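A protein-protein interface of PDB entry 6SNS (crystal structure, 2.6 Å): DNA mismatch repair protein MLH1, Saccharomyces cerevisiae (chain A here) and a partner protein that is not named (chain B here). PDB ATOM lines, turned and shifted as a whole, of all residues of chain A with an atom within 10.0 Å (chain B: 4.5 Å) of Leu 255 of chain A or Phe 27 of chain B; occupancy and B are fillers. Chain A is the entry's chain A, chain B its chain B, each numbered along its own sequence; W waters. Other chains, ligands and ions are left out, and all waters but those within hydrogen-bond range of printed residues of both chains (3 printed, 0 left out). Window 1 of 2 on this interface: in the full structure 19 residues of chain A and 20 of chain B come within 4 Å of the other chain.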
ATOM      1  N   ASN A  33     -15.257  -6.503 -28.143  1.00  0.00           N
ATOM      2  CA  ASN A  33     -15.478  -5.141 -27.682  1.00  0.00           C
ATOM      3  C   ASN A  33     -14.579  -4.979 -26.450  1.00  0.00           C
ATOM      4  O   ASN A  33     -14.954  -5.367 -25.336  1.00  0.00           O
ATOM      5  CB  ASN A  33     -16.957  -4.879 -27.380  1.00  0.00           C
ATOM      6  CG  ASN A  33     -17.261  -3.412 -27.263  1.00  0.00           C
ATOM      7  OD1 ASN A  33     -17.181  -2.817 -26.175  1.00  0.00           O
ATOM      8  ND2 ASN A  33     -17.594  -2.789 -28.390  1.00  0.00           N
ATOM      9  N   VAL A  35     -12.787  -3.920 -23.305  1.00  0.00           N
ATOM     10  CA  VAL A  35     -13.162  -3.214 -22.083  1.00  0.00           C
ATOM     11  C   VAL A  35     -11.891  -2.536 -21.512  1.00  0.00           C
ATOM     12  O   VAL A  35     -11.830  -1.299 -21.480  1.00  0.00           O
ATOM     13  CB  VAL A  35     -13.895  -4.156 -21.075  1.00  0.00           C
ATOM     14  CG1 VAL A  35     -14.202  -3.454 -19.745  1.00  0.00           C
ATOM     15  CG2 VAL A  35     -15.169  -4.749 -21.693  1.00  0.00           C
ATOM     16  N   ILE A  47     -12.520  -8.334 -22.681  1.00  0.00           N
ATOM     17  CA  ILE A  47     -13.274  -8.028 -23.899  1.00  0.00           C
ATOM     18  C   ILE A  47     -14.691  -8.536 -23.727  1.00  0.00           C
ATOM     19  O   ILE A  47     -14.924  -9.452 -22.930  1.00  0.00           O
ATOM     20  CB  ILE A  47     -12.626  -8.539 -25.224  1.00  0.00           C
ATOM     21  CG1 ILE A  47     -12.539 -10.083 -25.288  1.00  0.00           C
ATOM     22  CG2 ILE A  47     -11.275  -7.889 -25.491  1.00  0.00           C
ATOM     23  CD1 ILE A  47     -13.450 -10.743 -26.286  1.00  0.00           C
ATOM     24  N   GLN A  48     -15.633  -7.964 -24.476  1.00  0.00           N
ATOM     25  CA  GLN A  48     -17.005  -8.426 -24.420  1.00  0.00           C
ATOM     26  C   GLN A  48     -17.425  -8.962 -25.781  1.00  0.00           C
ATOM     27  O   GLN A  48     -17.370  -8.242 -26.779  1.00  0.00           O
ATOM     28  CB  GLN A  48     -17.945  -7.318 -23.933  1.00  0.00           C
ATOM     29  CG  GLN A  48     -19.347  -7.812 -23.596  1.00  0.00           C
ATOM     30  CD  GLN A  48     -20.330  -6.687 -23.593  1.00  0.00           C
ATOM     31  OE1 GLN A  48     -20.394  -5.896 -22.654  1.00  0.00           O
ATOM     32  NE2 GLN A  48     -21.118  -6.598 -24.647  1.00  0.00           N
ATOM     33  N   HIS A  49     -17.804 -10.243 -25.816  1.00  0.00           N
ATOM     34  CA  HIS A  49     -18.291 -10.902 -27.019  1.00  0.00           C
ATOM     35  C   HIS A  49     -19.754 -11.223 -26.764  1.00  0.00           C
ATOM     36  O   HIS A  49     -20.065 -11.988 -25.844  1.00  0.00           O
ATOM     37  CB  HIS A  49     -17.469 -12.153 -27.355  1.00  0.00           C
ATOM     38  CG  HIS A  49     -18.078 -12.994 -28.433  1.00  0.00           C
ATOM     39  ND1 HIS A  49     -18.106 -12.570 -29.751  1.00  0.00           N
ATOM     40  CD2 HIS A  49     -18.680 -14.201 -28.349  1.00  0.00           C
ATOM     41  CE1 HIS A  49     -18.716 -13.532 -30.422  1.00  0.00           C
ATOM     42  NE2 HIS A  49     -19.071 -14.537 -29.622  1.00  0.00           N
ATOM     43  N   ASP A  50     -20.648 -10.583 -27.551  1.00  0.00           N
ATOM     44  CA  ASP A  50     -22.107 -10.663 -27.444  1.00  0.00           C
ATOM     45  C   ASP A  50     -22.523 -10.148 -26.059  1.00  0.00           C
ATOM     46  O   ASP A  50     -22.301  -8.969 -25.771  1.00  0.00           O
ATOM     47  CB  ASP A  50     -22.644 -12.082 -27.755  1.00  0.00           C
ATOM     48  CG  ASP A  50     -22.268 -12.600 -29.129  1.00  0.00           C
ATOM     49  OD1 ASP A  50     -22.519 -11.885 -30.127  1.00  0.00           O
ATOM     50  OD2 ASP A  50     -21.734 -13.723 -29.209  1.00  0.00           O
ATOM     51  N   LEU A  51     -23.056 -11.029 -25.194  1.00  0.00           N
ATOM     52  CA  LEU A  51     -23.463 -10.678 -23.838  1.00  0.00           C
ATOM     53  C   LEU A  51     -22.605 -11.425 -22.815  1.00  0.00           C
ATOM     54  O   LEU A  51     -23.043 -11.683 -21.693  1.00  0.00           O
ATOM     55  CB  LEU A  51     -24.959 -10.954 -23.637  1.00  0.00           C
ATOM     56  CG  LEU A  51     -25.897  -9.905 -24.210  1.00  0.00           C
ATOM     57  CD1 LEU A  51     -26.408 -10.316 -25.592  1.00  0.00           C
ATOM     58  CD2 LEU A  51     -27.059  -9.678 -23.287  1.00  0.00           C
ATOM     59  N   LYS A  52     -21.364 -11.762 -23.213  1.00  0.00           N
ATOM     60  CA  LYS A  52     -20.400 -12.469 -22.375  1.00  0.00           C
ATOM     61  C   LYS A  52     -19.157 -11.631 -22.214  1.00  0.00           C
ATOM     62  O   LYS A  52     -18.694 -11.014 -23.174  1.00  0.00           O
ATOM     63  CB  LYS A  52     -20.026 -13.838 -22.979  1.00  0.00           C
ATOM     64  CG  LYS A  52     -21.030 -14.954 -22.704  1.00  0.00           C
ATOM     65  CD  LYS A  52     -20.653 -16.229 -23.440  1.00  0.00           C
ATOM     66  CE  LYS A  52     -21.682 -17.317 -23.261  1.00  0.00           C
ATOM     67  NZ  LYS A  52     -21.306 -18.550 -24.002  1.00  0.00           N
ATOM     68  N   LEU A  53     -18.610 -11.634 -20.997  1.00  0.00           N
ATOM     69  CA  LEU A  53     -17.378 -10.942 -20.641  1.00  0.00           C
ATOM     70  C   LEU A  53     -16.241 -11.970 -20.558  1.00  0.00           C
ATOM     71  O   LEU A  53     -16.360 -12.979 -19.856  1.00  0.00           O
ATOM     72  CB  LEU A  53     -17.557 -10.202 -19.311  1.00  0.00           C
ATOM     73  CG  LEU A  53     -16.617  -9.040 -19.077  1.00  0.00           C
ATOM     74  CD1 LEU A  53     -16.991  -7.851 -19.944  1.00  0.00           C
ATOM     75  CD2 LEU A  53     -16.596  -8.658 -17.624  1.00  0.00           C
ATOM     76  N   PHE A  54     -15.164 -11.726 -21.321  1.00  0.00           N
ATOM     77  CA  PHE A  54     -14.006 -12.613 -21.405  1.00  0.00           C
ATOM     78  C   PHE A  54     -12.725 -12.037 -20.818  1.00  0.00           C
ATOM     79  O   PHE A  54     -12.558 -10.817 -20.793  1.00  0.00           O
ATOM     80  CB  PHE A  54     -13.764 -13.041 -22.864  1.00  0.00           C
ATOM     81  CG  PHE A  54     -14.793 -14.015 -23.375  1.00  0.00           C
ATOM     82  CD1 PHE A  54     -14.741 -15.359 -23.019  1.00  0.00           C
ATOM     83  CD2 PHE A  54     -15.825 -13.591 -24.203  1.00  0.00           C
ATOM     84  CE1 PHE A  54     -15.710 -16.257 -23.471  1.00  0.00           C
ATOM     85  CE2 PHE A  54     -16.786 -14.495 -24.668  1.00  0.00           C
ATOM     86  CZ  PHE A  54     -16.721 -15.821 -24.300  1.00  0.00           C
ATOM     87  N   GLU A 251     -14.067 -17.375 -19.931  1.00  0.00           N
ATOM     88  CA  GLU A 251     -15.321 -16.682 -19.671  1.00  0.00           C
ATOM     89  C   GLU A 251     -15.321 -16.330 -18.178  1.00  0.00           C
ATOM     90  O   GLU A 251     -15.019 -17.192 -17.352  1.00  0.00           O
ATOM     91  CB  GLU A 251     -16.532 -17.561 -20.034  1.00  0.00           C
ATOM     92  CG  GLU A 251     -17.827 -16.774 -20.163  1.00  0.00           C
ATOM     93  CD  GLU A 251     -19.110 -17.583 -20.229  1.00  0.00           C
ATOM     94  OE1 GLU A 251     -19.972 -17.394 -19.338  1.00  0.00           O
ATOM     95  OE2 GLU A 251     -19.262 -18.392 -21.175  1.00  0.00           O
ATOM     96  N   ILE A 252     -15.597 -15.066 -17.836  1.00  0.00           N
ATOM     97  CA  ILE A 252     -15.626 -14.620 -16.438  1.00  0.00           C
ATOM     98  C   ILE A 252     -17.037 -14.206 -16.018  1.00  0.00           C
ATOM     99  O   ILE A 252     -17.403 -14.351 -14.846  1.00  0.00           O
ATOM    100  CB  ILE A 252     -14.555 -13.548 -16.106  1.00  0.00           C
ATOM    101  CG1 ILE A 252     -14.566 -12.372 -17.122  1.00  0.00           C
ATOM    102  CG2 ILE A 252     -13.181 -14.205 -15.980  1.00  0.00           C
ATOM    103  CD1 ILE A 252     -13.724 -11.149 -16.760  1.00  0.00           C
ATOM    104  N   ALA A 253     -17.838 -13.719 -16.983  1.00  0.00           N
ATOM    105  CA  ALA A 253     -19.216 -13.324 -16.739  1.00  0.00           C
ATOM    106  C   ALA A 253     -20.130 -13.522 -17.949  1.00  0.00           C
ATOM    107  O   ALA A 253     -19.726 -13.306 -19.094  1.00  0.00           O
ATOM    108  CB  ALA A 253     -19.274 -11.878 -16.277  1.00  0.00           C
ATOM    109  N   ASN A 254     -21.367 -13.962 -17.672  1.00  0.00           N
ATOM    110  CA  ASN A 254     -22.452 -14.083 -18.637  1.00  0.00           C
ATOM    111  C   ASN A 254     -23.423 -12.984 -18.184  1.00  0.00           C
ATOM    112  O   ASN A 254     -24.087 -13.126 -17.152  1.00  0.00           O
ATOM    113  CB  ASN A 254     -23.096 -15.473 -18.612  1.00  0.00           C
ATOM    114  CG  ASN A 254     -24.169 -15.672 -19.666  1.00  0.00           C
ATOM    115  OD1 ASN A 254     -24.083 -15.181 -20.802  1.00  0.00           O
ATOM    116  ND2 ASN A 254     -25.205 -16.413 -19.317  1.00  0.00           N
ATOM    117  N   LEU A 255     -23.412 -11.847 -18.910  1.00  0.00           N
ATOM    118  CA  LEU A 255     -24.161 -10.622 -18.620  1.00  0.00           C
ATOM    119  C   LEU A 255     -25.701 -10.771 -18.526  1.00  0.00           C
ATOM    120  O   LEU A 255     -26.242 -10.090 -17.653  1.00  0.00           O
ATOM    121  CB  LEU A 255     -23.787  -9.508 -19.597  1.00  0.00           C
ATOM    122  CG  LEU A 255     -22.296  -9.143 -19.639  1.00  0.00           C
ATOM    123  CD1 LEU A 255     -21.962  -8.404 -20.898  1.00  0.00           C
ATOM    124  CD2 LEU A 255     -21.870  -8.346 -18.411  1.00  0.00           C
ATOM    125  N   PRO A 256     -26.448 -11.623 -19.301  1.00  0.00           N
ATOM    126  CA  PRO A 256     -27.904 -11.731 -19.060  1.00  0.00           C
ATOM    127  C   PRO A 256     -28.244 -12.309 -17.679  1.00  0.00           C
ATOM    128  O   PRO A 256     -29.319 -12.019 -17.152  1.00  0.00           O
ATOM    129  CB  PRO A 256     -28.403 -12.638 -20.192  1.00  0.00           C
ATOM    130  CG  PRO A 256     -27.296 -12.712 -21.168  1.00  0.00           C
ATOM    131  CD  PRO A 256     -26.038 -12.528 -20.394  1.00  0.00           C
ATOM    132  N   ASP A 257     -27.306 -13.089 -17.080  1.00  0.00           N
ATOM    133  CA  ASP A 257     -27.425 -13.677 -15.740  1.00  0.00           C
ATOM    134  C   ASP A 257     -27.276 -12.596 -14.659  1.00  0.00           C
ATOM    135  O   ASP A 257     -27.627 -12.830 -13.502  1.00  0.00           O
ATOM    136  CB  ASP A 257     -26.363 -14.780 -15.525  1.00  0.00           C
ATOM    137  CG  ASP A 257     -26.477 -16.021 -16.400  1.00  0.00           C
ATOM    138  OD1 ASP A 257     -27.508 -16.173 -17.096  1.00  0.00           O
ATOM    139  OD2 ASP A 257     -25.534 -16.846 -16.384  1.00  0.00           O
ATOM    140  N   LEU A 258     -26.742 -11.422 -15.046  1.00  0.00           N
ATOM    141  CA  LEU A 258     -26.512 -10.265 -14.183  1.00  0.00           C
ATOM    142  C   LEU A 258     -27.655  -9.244 -14.229  1.00  0.00           C
ATOM    143  O   LEU A 258     -27.784  -8.448 -13.296  1.00  0.00           O
ATOM    144  CB  LEU A 258     -25.162  -9.601 -14.524  1.00  0.00           C
ATOM    145  CG  LEU A 258     -23.932  -9.908 -13.638  1.00  0.00           C
ATOM    146  CD1 LEU A 258     -24.062  -9.293 -12.246  1.00  0.00           C
ATOM    147  CD2 LEU A 258     -23.582 -11.400 -13.603  1.00  0.00           C
ATOM    148  N   TYR A 259     -28.490  -9.274 -15.301  1.00  0.00           N
ATOM    149  CA  TYR A 259     -29.671  -8.406 -15.463  1.00  0.00           C
ATOM    150  C   TYR A 259     -30.744  -8.827 -14.452  1.00  0.00           C
ATOM    151  O   TYR A 259     -31.545  -7.996 -14.020  1.00  0.00           O
ATOM    152  CB  TYR A 259     -30.297  -8.562 -16.865  1.00  0.00           C
ATOM    153  CG  TYR A 259     -29.467  -8.189 -18.078  1.00  0.00           C
ATOM    154  CD1 TYR A 259     -28.412  -7.282 -17.980  1.00  0.00           C
ATOM    155  CD2 TYR A 259     -29.808  -8.654 -19.346  1.00  0.00           C
ATOM    156  CE1 TYR A 259     -27.660  -6.926 -19.098  1.00  0.00           C
ATOM    157  CE2 TYR A 259     -29.076  -8.289 -20.473  1.00  0.00           C
ATOM    158  CZ  TYR A 259     -28.011  -7.418 -20.347  1.00  0.00           C
ATOM    159  OH  TYR A 259     -27.312  -7.044 -21.465  1.00  0.00           O
ATOM    160  N   LYS A 260     -30.787 -10.147 -14.144  1.00  0.00           N
ATOM    161  CA  LYS A 260     -31.702 -10.828 -13.219  1.00  0.00           C
ATOM    162  C   LYS A 260     -31.557 -10.302 -11.783  1.00  0.00           C
ATOM    163  O   LYS A 260     -32.567 -10.143 -11.089  1.00  0.00           O
ATOM    164  CB  LYS A 260     -31.439 -12.350 -13.260  1.00  0.00           C
ATOM    165  CG  LYS A 260     -32.492 -13.207 -12.565  1.00  0.00           C
ATOM    166  CD  LYS A 260     -32.111 -14.680 -12.598  1.00  0.00           C
ATOM    167  CE  LYS A 260     -33.218 -15.567 -12.086  1.00  0.00           C
ATOM    168  NZ  LYS A 260     -32.905 -17.006 -12.291  1.00  0.00           N
ATOM    169  N   VAL A 261     -30.299 -10.045 -11.350  1.00  0.00           N
ATOM    170  CA  VAL A 261     -29.937  -9.552 -10.014  1.00  0.00           C
ATOM    171  C   VAL A 261     -30.557  -8.169  -9.734  1.00  0.00           C
ATOM    172  O   VAL A 261     -30.950  -7.900  -8.596  1.00  0.00           O
ATOM    173  CB  VAL A 261     -28.396  -9.553  -9.767  1.00  0.00           C
ATOM    174  CG1 VAL A 261     -28.075  -9.526  -8.272  1.00  0.00           C
ATOM    175  CG2 VAL A 261     -27.711 -10.749 -10.437  1.00  0.00           C
ATOM    176  N   PHE A 262     -30.646  -7.303 -10.773  1.00  0.00           N
ATOM    177  CA  PHE A 262     -31.190  -5.941 -10.671  1.00  0.00           C
ATOM    178  C   PHE A 262     -31.999  -5.514 -11.908  1.00  0.00           C
ATOM    179  O   PHE A 262     -31.429  -5.284 -12.978  1.00  0.00           O
ATOM    180  CB  PHE A 262     -30.088  -4.903 -10.336  1.00  0.00           C
ATOM    181  CG  PHE A 262     -28.658  -5.404 -10.253  1.00  0.00           C
ATOM    182  CD1 PHE A 262     -27.878  -5.530 -11.397  1.00  0.00           C
ATOM    183  CD2 PHE A 262     -28.090  -5.736  -9.029  1.00  0.00           C
ATOM    184  CE1 PHE A 262     -26.559  -5.991 -11.319  1.00  0.00           C
ATOM    185  CE2 PHE A 262     -26.766  -6.186  -8.951  1.00  0.00           C
ATOM    186  CZ  PHE A 262     -26.010  -6.308 -10.096  1.00  0.00           C
ATOM    187  N   GLU A 263     -33.328  -5.401 -11.746  1.00  0.00           N
ATOM    188  CA  GLU A 263     -34.254  -4.985 -12.803  1.00  0.00           C
ATOM    189  C   GLU A 263     -34.639  -3.501 -12.631  1.00  0.00           C
ATOM    190  O   GLU A 263     -34.620  -2.999 -11.500  1.00  0.00           O
ATOM    191  CB  GLU A 263     -35.493  -5.914 -12.818  1.00  0.00           C
ATOM    192  CG  GLU A 263     -36.562  -5.632 -13.874  1.00  0.00           C
ATOM    193  CD  GLU A 263     -36.136  -5.518 -15.328  1.00  0.00           C
ATOM    194  OE1 GLU A 263     -35.250  -6.289 -15.764  1.00  0.00           O
ATOM    195  OE2 GLU A 263     -36.707  -4.657 -16.037  1.00  0.00           O
ATOM    196  N   GLN B  22     -16.661   1.112 -18.463  1.00  0.00           N
ATOM    197  CA  GLN B  22     -18.088   0.777 -18.549  1.00  0.00           C
ATOM    198  C   GLN B  22     -18.321  -0.490 -19.400  1.00  0.00           C
ATOM    199  O   GLN B  22     -17.679  -0.682 -20.439  1.00  0.00           O
ATOM    200  CB  GLN B  22     -18.885   1.974 -19.088  1.00  0.00           C
ATOM    201  CG  GLN B  22     -20.363   1.704 -19.368  1.00  0.00           C
ATOM    202  CD  GLN B  22     -21.100   2.961 -19.748  1.00  0.00           C
ATOM    203  OE1 GLN B  22     -20.750   3.676 -20.691  1.00  0.00           O
ATOM    204  NE2 GLN B  22     -22.151   3.254 -19.017  1.00  0.00           N
ATOM    205  N   VAL B  23     -19.233  -1.356 -18.940  1.00  0.00           N
ATOM    206  CA  VAL B  23     -19.556  -2.616 -19.608  1.00  0.00           C
ATOM    207  C   VAL B  23     -21.043  -2.655 -19.962  1.00  0.00           C
ATOM    208  O   VAL B  23     -21.877  -2.683 -19.055  1.00  0.00           O
ATOM    209  CB  VAL B  23     -19.172  -3.839 -18.730  1.00  0.00           C
ATOM    210  CG1 VAL B  23     -19.435  -5.140 -19.469  1.00  0.00           C
ATOM    211  CG2 VAL B  23     -17.730  -3.771 -18.259  1.00  0.00           C
ATOM    212  N   ASP B  24     -21.367  -2.696 -21.276  1.00  0.00           N
ATOM    213  CA  ASP B  24     -22.729  -2.825 -21.824  1.00  0.00           C
ATOM    214  C   ASP B  24     -23.640  -1.632 -21.498  1.00  0.00           C
ATOM    215  O   ASP B  24     -24.869  -1.748 -21.578  1.00  0.00           O
ATOM    216  CB  ASP B  24     -23.363  -4.158 -21.339  1.00  0.00           C
ATOM    217  CG  ASP B  24     -24.419  -4.784 -22.229  1.00  0.00           C
ATOM    218  OD1 ASP B  24     -24.686  -4.233 -23.330  1.00  0.00           O
ATOM    219  OD2 ASP B  24     -24.974  -5.826 -21.837  1.00  0.00           O
ATOM    220  N   LYS B  25     -23.036  -0.468 -21.175  1.00  0.00           N
ATOM    221  CA  LYS B  25     -23.725   0.754 -20.731  1.00  0.00           C
ATOM    222  C   LYS B  25     -24.685   0.443 -19.550  1.00  0.00           C
ATOM    223  O   LYS B  25     -25.702   1.111 -19.375  1.00  0.00           O
ATOM    224  CB  LYS B  25     -24.407   1.593 -21.856  1.00  0.00           C
ATOM    225  CG  LYS B  25     -24.333   1.098 -23.291  1.00  0.00           C
ATOM    226  CD  LYS B  25     -23.154   1.682 -24.024  1.00  0.00           C
ATOM    227  CE  LYS B  25     -23.225   1.409 -25.508  1.00  0.00           C
ATOM    228  NZ  LYS B  25     -22.929  -0.015 -25.847  1.00  0.00           N
ATOM    229  N   LYS B  26     -24.331  -0.571 -18.737  1.00  0.00           N
ATOM    230  CA  LYS B  26     -25.102  -1.010 -17.572  1.00  0.00           C
ATOM    231  C   LYS B  26     -24.227  -1.107 -16.317  1.00  0.00           C
ATOM    232  O   LYS B  26     -24.662  -0.704 -15.234  1.00  0.00           O
ATOM    233  CB  LYS B  26     -25.807  -2.349 -17.847  1.00  0.00           C
ATOM    234  CG  LYS B  26     -26.935  -2.215 -18.858  1.00  0.00           C
ATOM    235  CD  LYS B  26     -27.593  -3.540 -19.182  1.00  0.00           C
ATOM    236  CE  LYS B  26     -28.734  -3.393 -20.163  1.00  0.00           C
ATOM    237  NZ  LYS B  26     -28.256  -3.161 -21.556  1.00  0.00           N
ATOM    238  N   PHE B  27     -22.993  -1.620 -16.469  1.00  0.00           N
ATOM    239  CA  PHE B  27     -22.062  -1.828 -15.364  1.00  0.00           C
ATOM    240  C   PHE B  27     -20.791  -1.033 -15.491  1.00  0.00           C
ATOM    241  O   PHE B  27     -20.489  -0.482 -16.547  1.00  0.00           O
ATOM    242  CB  PHE B  27     -21.694  -3.318 -15.263  1.00  0.00           C
ATOM    243  CG  PHE B  27     -22.860  -4.276 -15.348  1.00  0.00           C
ATOM    244  CD1 PHE B  27     -23.688  -4.488 -14.253  1.00  0.00           C
ATOM    245  CD2 PHE B  27     -23.124  -4.971 -16.522  1.00  0.00           C
ATOM    246  CE1 PHE B  27     -24.764  -5.366 -14.337  1.00  0.00           C
ATOM    247  CE2 PHE B  27     -24.204  -5.848 -16.605  1.00  0.00           C
ATOM    248  CZ  PHE B  27     -25.019  -6.036 -15.513  1.00  0.00           C
ATOM    249  N   ILE B  28     -20.028  -0.991 -14.406  1.00  0.00           N
ATOM    250  CA  ILE B  28     -18.708  -0.375 -14.361  1.00  0.00           C
ATOM    251  C   ILE B  28     -17.788  -1.486 -13.837  1.00  0.00           C
ATOM    252  O   ILE B  28     -17.949  -1.899 -12.675  1.00  0.00           O
ATOM    253  CB  ILE B  28     -18.682   0.901 -13.474  1.00  0.00           C
ATOM    254  CG1 ILE B  28     -19.523   2.045 -14.106  1.00  0.00           C
ATOM    255  CG2 ILE B  28     -17.233   1.348 -13.192  1.00  0.00           C
ATOM    256  CD1 ILE B  28     -20.142   3.006 -13.094  1.00  0.00           C
ATOM    257  N   LEU B  29     -16.881  -2.022 -14.701  1.00  0.00           N
ATOM    258  CA  LEU B  29     -15.970  -3.091 -14.279  1.00  0.00           C
ATOM    259  C   LEU B  29     -14.816  -2.526 -13.490  1.00  0.00           C
ATOM    260  O   LEU B  29     -14.110  -1.653 -13.983  1.00  0.00           O
ATOM    261  CB  LEU B  29     -15.465  -3.954 -15.450  1.00  0.00           C
ATOM    262  CG  LEU B  29     -14.594  -5.183 -15.122  1.00  0.00           C
ATOM    263  CD1 LEU B  29     -15.283  -6.151 -14.153  1.00  0.00           C
ATOM    264  CD2 LEU B  29     -14.221  -5.908 -16.379  1.00  0.00           C
ATOM    265  N   LEU B  45     -18.461  -6.169 -10.969  1.00  0.00           N
ATOM    266  CA  LEU B  45     -19.273  -5.348 -11.863  1.00  0.00           C
ATOM    267  C   LEU B  45     -20.225  -4.544 -10.970  1.00  0.00           C
ATOM    268  O   LEU B  45     -21.053  -5.121 -10.262  1.00  0.00           O
ATOM    269  CB  LEU B  45     -20.057  -6.186 -12.901  1.00  0.00           C
ATOM    270  CG  LEU B  45     -19.267  -6.764 -14.081  1.00  0.00           C
ATOM    271  CD1 LEU B  45     -20.054  -7.860 -14.765  1.00  0.00           C
ATOM    272  CD2 LEU B  45     -18.877  -5.682 -15.096  1.00  0.00           C
ATOM    273  N   VAL B  46     -20.046  -3.224 -10.944  1.00  0.00           N
ATOM    274  CA  VAL B  46     -20.871  -2.310 -10.157  1.00  0.00           C
ATOM    275  C   VAL B  46     -22.034  -1.841 -11.049  1.00  0.00           C
ATOM    276  O   VAL B  46     -21.793  -1.334 -12.149  1.00  0.00           O
ATOM    277  CB  VAL B  46     -20.034  -1.117  -9.622  1.00  0.00           C
ATOM    278  CG1 VAL B  46     -20.896  -0.148  -8.827  1.00  0.00           C
ATOM    279  CG2 VAL B  46     -18.854  -1.597  -8.787  1.00  0.00           C
ATOM    280  N   ASP B  47     -23.290  -2.031 -10.584  1.00  0.00           N
ATOM    281  CA  ASP B  47     -24.501  -1.592 -11.295  1.00  0.00           C
ATOM    282  C   ASP B  47     -24.469  -0.054 -11.304  1.00  0.00           C
ATOM    283  O   ASP B  47     -24.511   0.566 -10.233  1.00  0.00           O
ATOM    284  CB  ASP B  47     -25.759  -2.133 -10.585  1.00  0.00           C
ATOM    285  CG  ASP B  47     -27.103  -1.733 -11.171  1.00  0.00           C
ATOM    286  OD1 ASP B  47     -27.137  -0.820 -12.018  1.00  0.00           O
ATOM    287  OD2 ASP B  47     -28.123  -2.315 -10.760  1.00  0.00           O
ATOM    288  N   GLN B  48     -24.342   0.550 -12.503  1.00  0.00           N
ATOM    289  CA  GLN B  48     -24.201   1.999 -12.637  1.00  0.00           C
ATOM    290  C   GLN B  48     -25.369   2.781 -12.054  1.00  0.00           C
ATOM    291  O   GLN B  48     -25.127   3.800 -11.407  1.00  0.00           O
ATOM    292  CB  GLN B  48     -23.899   2.431 -14.088  1.00  0.00           C
ATOM    293  CG  GLN B  48     -25.064   2.361 -15.078  1.00  0.00           C
ATOM    294  CD  GLN B  48     -24.611   2.584 -16.489  1.00  0.00           C
ATOM    295  OE1 GLN B  48     -23.641   1.983 -16.965  1.00  0.00           O
ATOM    296  NE2 GLN B  48     -25.307   3.457 -17.193  1.00  0.00           N
HETATM  297  O   HOH W   1     -19.155  -3.253 -23.577  1.00  0.00           O
HETATM  298  O   HOH W   2     -27.487  -5.676 -24.654  1.00  0.00           O
HETATM  299  O   HOH W   3     -16.889  -1.751 -23.552  1.00  0.00           O
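The side-chain hydroxyl of Tyr 259 of chain A sits at hydrogen-bond distance from the side-chain carboxylate of Asp 24 of chain B (2.7 Å).
Among the printed residues, pairs that only touch across the chains: Phe 262 of chain A with Asp 47 of chain B, Tyr 259 of chain A with Lys 26 of chain B, Gln 48 of chain A with Val 23 of chain B, Phe 262 of chain A with Phe 27 of chain B, Gln 48 of chain A with Asp 24 of chain B, Leu 53 of chain A with Val 23 of chain B, Leu 258 of chain A with Phe 27 of chain B, Leu 53 of chain A with Leu 29 of chain B, Val 35 of chain A with Val 23 of chain B and Leu 255 of chain A with Phe 27 of chain B.
Leu 255 of chain A touches just one residue of chain B: Phe 27. Phe 27 of chain B touches three residues of chain A. Of the printed residues of chain A, Val 23 of chain B touches Val 35 (3.8 Å), Gln 48 (3.4 Å) and Leu 53 (3.7 Å). Asp 24 of chain B touches just these residues of chain A: Gln 48 and Tyr 259. No residue of chain A comes within 4 Å of Ile 28 of chain B. Of the printed residues of chain B, Leu 258 of chain A touches Phe 27 (3.7 Å). Of the printed residues of chain B, Phe 262 of chain A touches Phe 27 (3.6 Å) and Asp 47 (3.2 Å). Of the printed residues of chain B, Leu 53 of chain A touches Val 23 and Leu 29. Of the printed residues of chain B, Tyr 259 of chain A touches Asp 24 and Lys 26. The nearest printed residue of chain B that does not touch Leu 255 of chain A is Asp 24 of chain B (4.1 Å). The nearest residue of chain A that does not touch Phe 27 of chain B is Tyr 259 of chain A (4.4 Å).
Along chain B the printed residues that touch a printed residue of chain A span positions 23 to 47. Of the 23 printed residues of chain A, 7 touch a printed residue of chain B.
Water W3 bridges OD1 of Asn 33 of chain A (2.8 Å) and O of Gln 22 of chain B (3.4 Å). Water W1 lies within hydrogen-bond range of the side-chain amide oxygen of Gln 48 of chain A, the backbone NH of Asp 24 of chain B and the side-chain amide oxygen of Asn 33 of chain A. Water W2 bridges OD1 of Asp 24 of chain B (3.4 Å) and OH of Tyr 259 of chain A (3.5 Å).
O of Asn 33 of chain A sits at hydrogen-bond distance from N of Gln 48 of chain A. The side-chain amide nitrogen (NE2) of Gln 48 of chain A is in hydrogen-bond range of the backbone carbonyl oxygen (O) of Asp 50 of chain A (2.9 Å). The backbone carbonyl oxygen (O) of Ala 253 of chain A is in hydrogen-bond range of the backbone NH (N) of Leu 53 of chain A (2.8 Å). The backbone carbonyl oxygen of Leu 53 of chain A is in hydrogen-bond range of the backbone NH of Ile 252 of chain A, at 3.0 Å. The backbone carbonyl oxygen (O) of Lys 26 of chain B sits at hydrogen-bond distance from the backbone NH (N) of Gln 48 of chain B (3.0 Å). The backbone carbonyl oxygen (O) of Leu 51 of chain A sits at hydrogen-bond distance from the backbone NH (N) of Leu 255 of chain A (2.8 Å).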
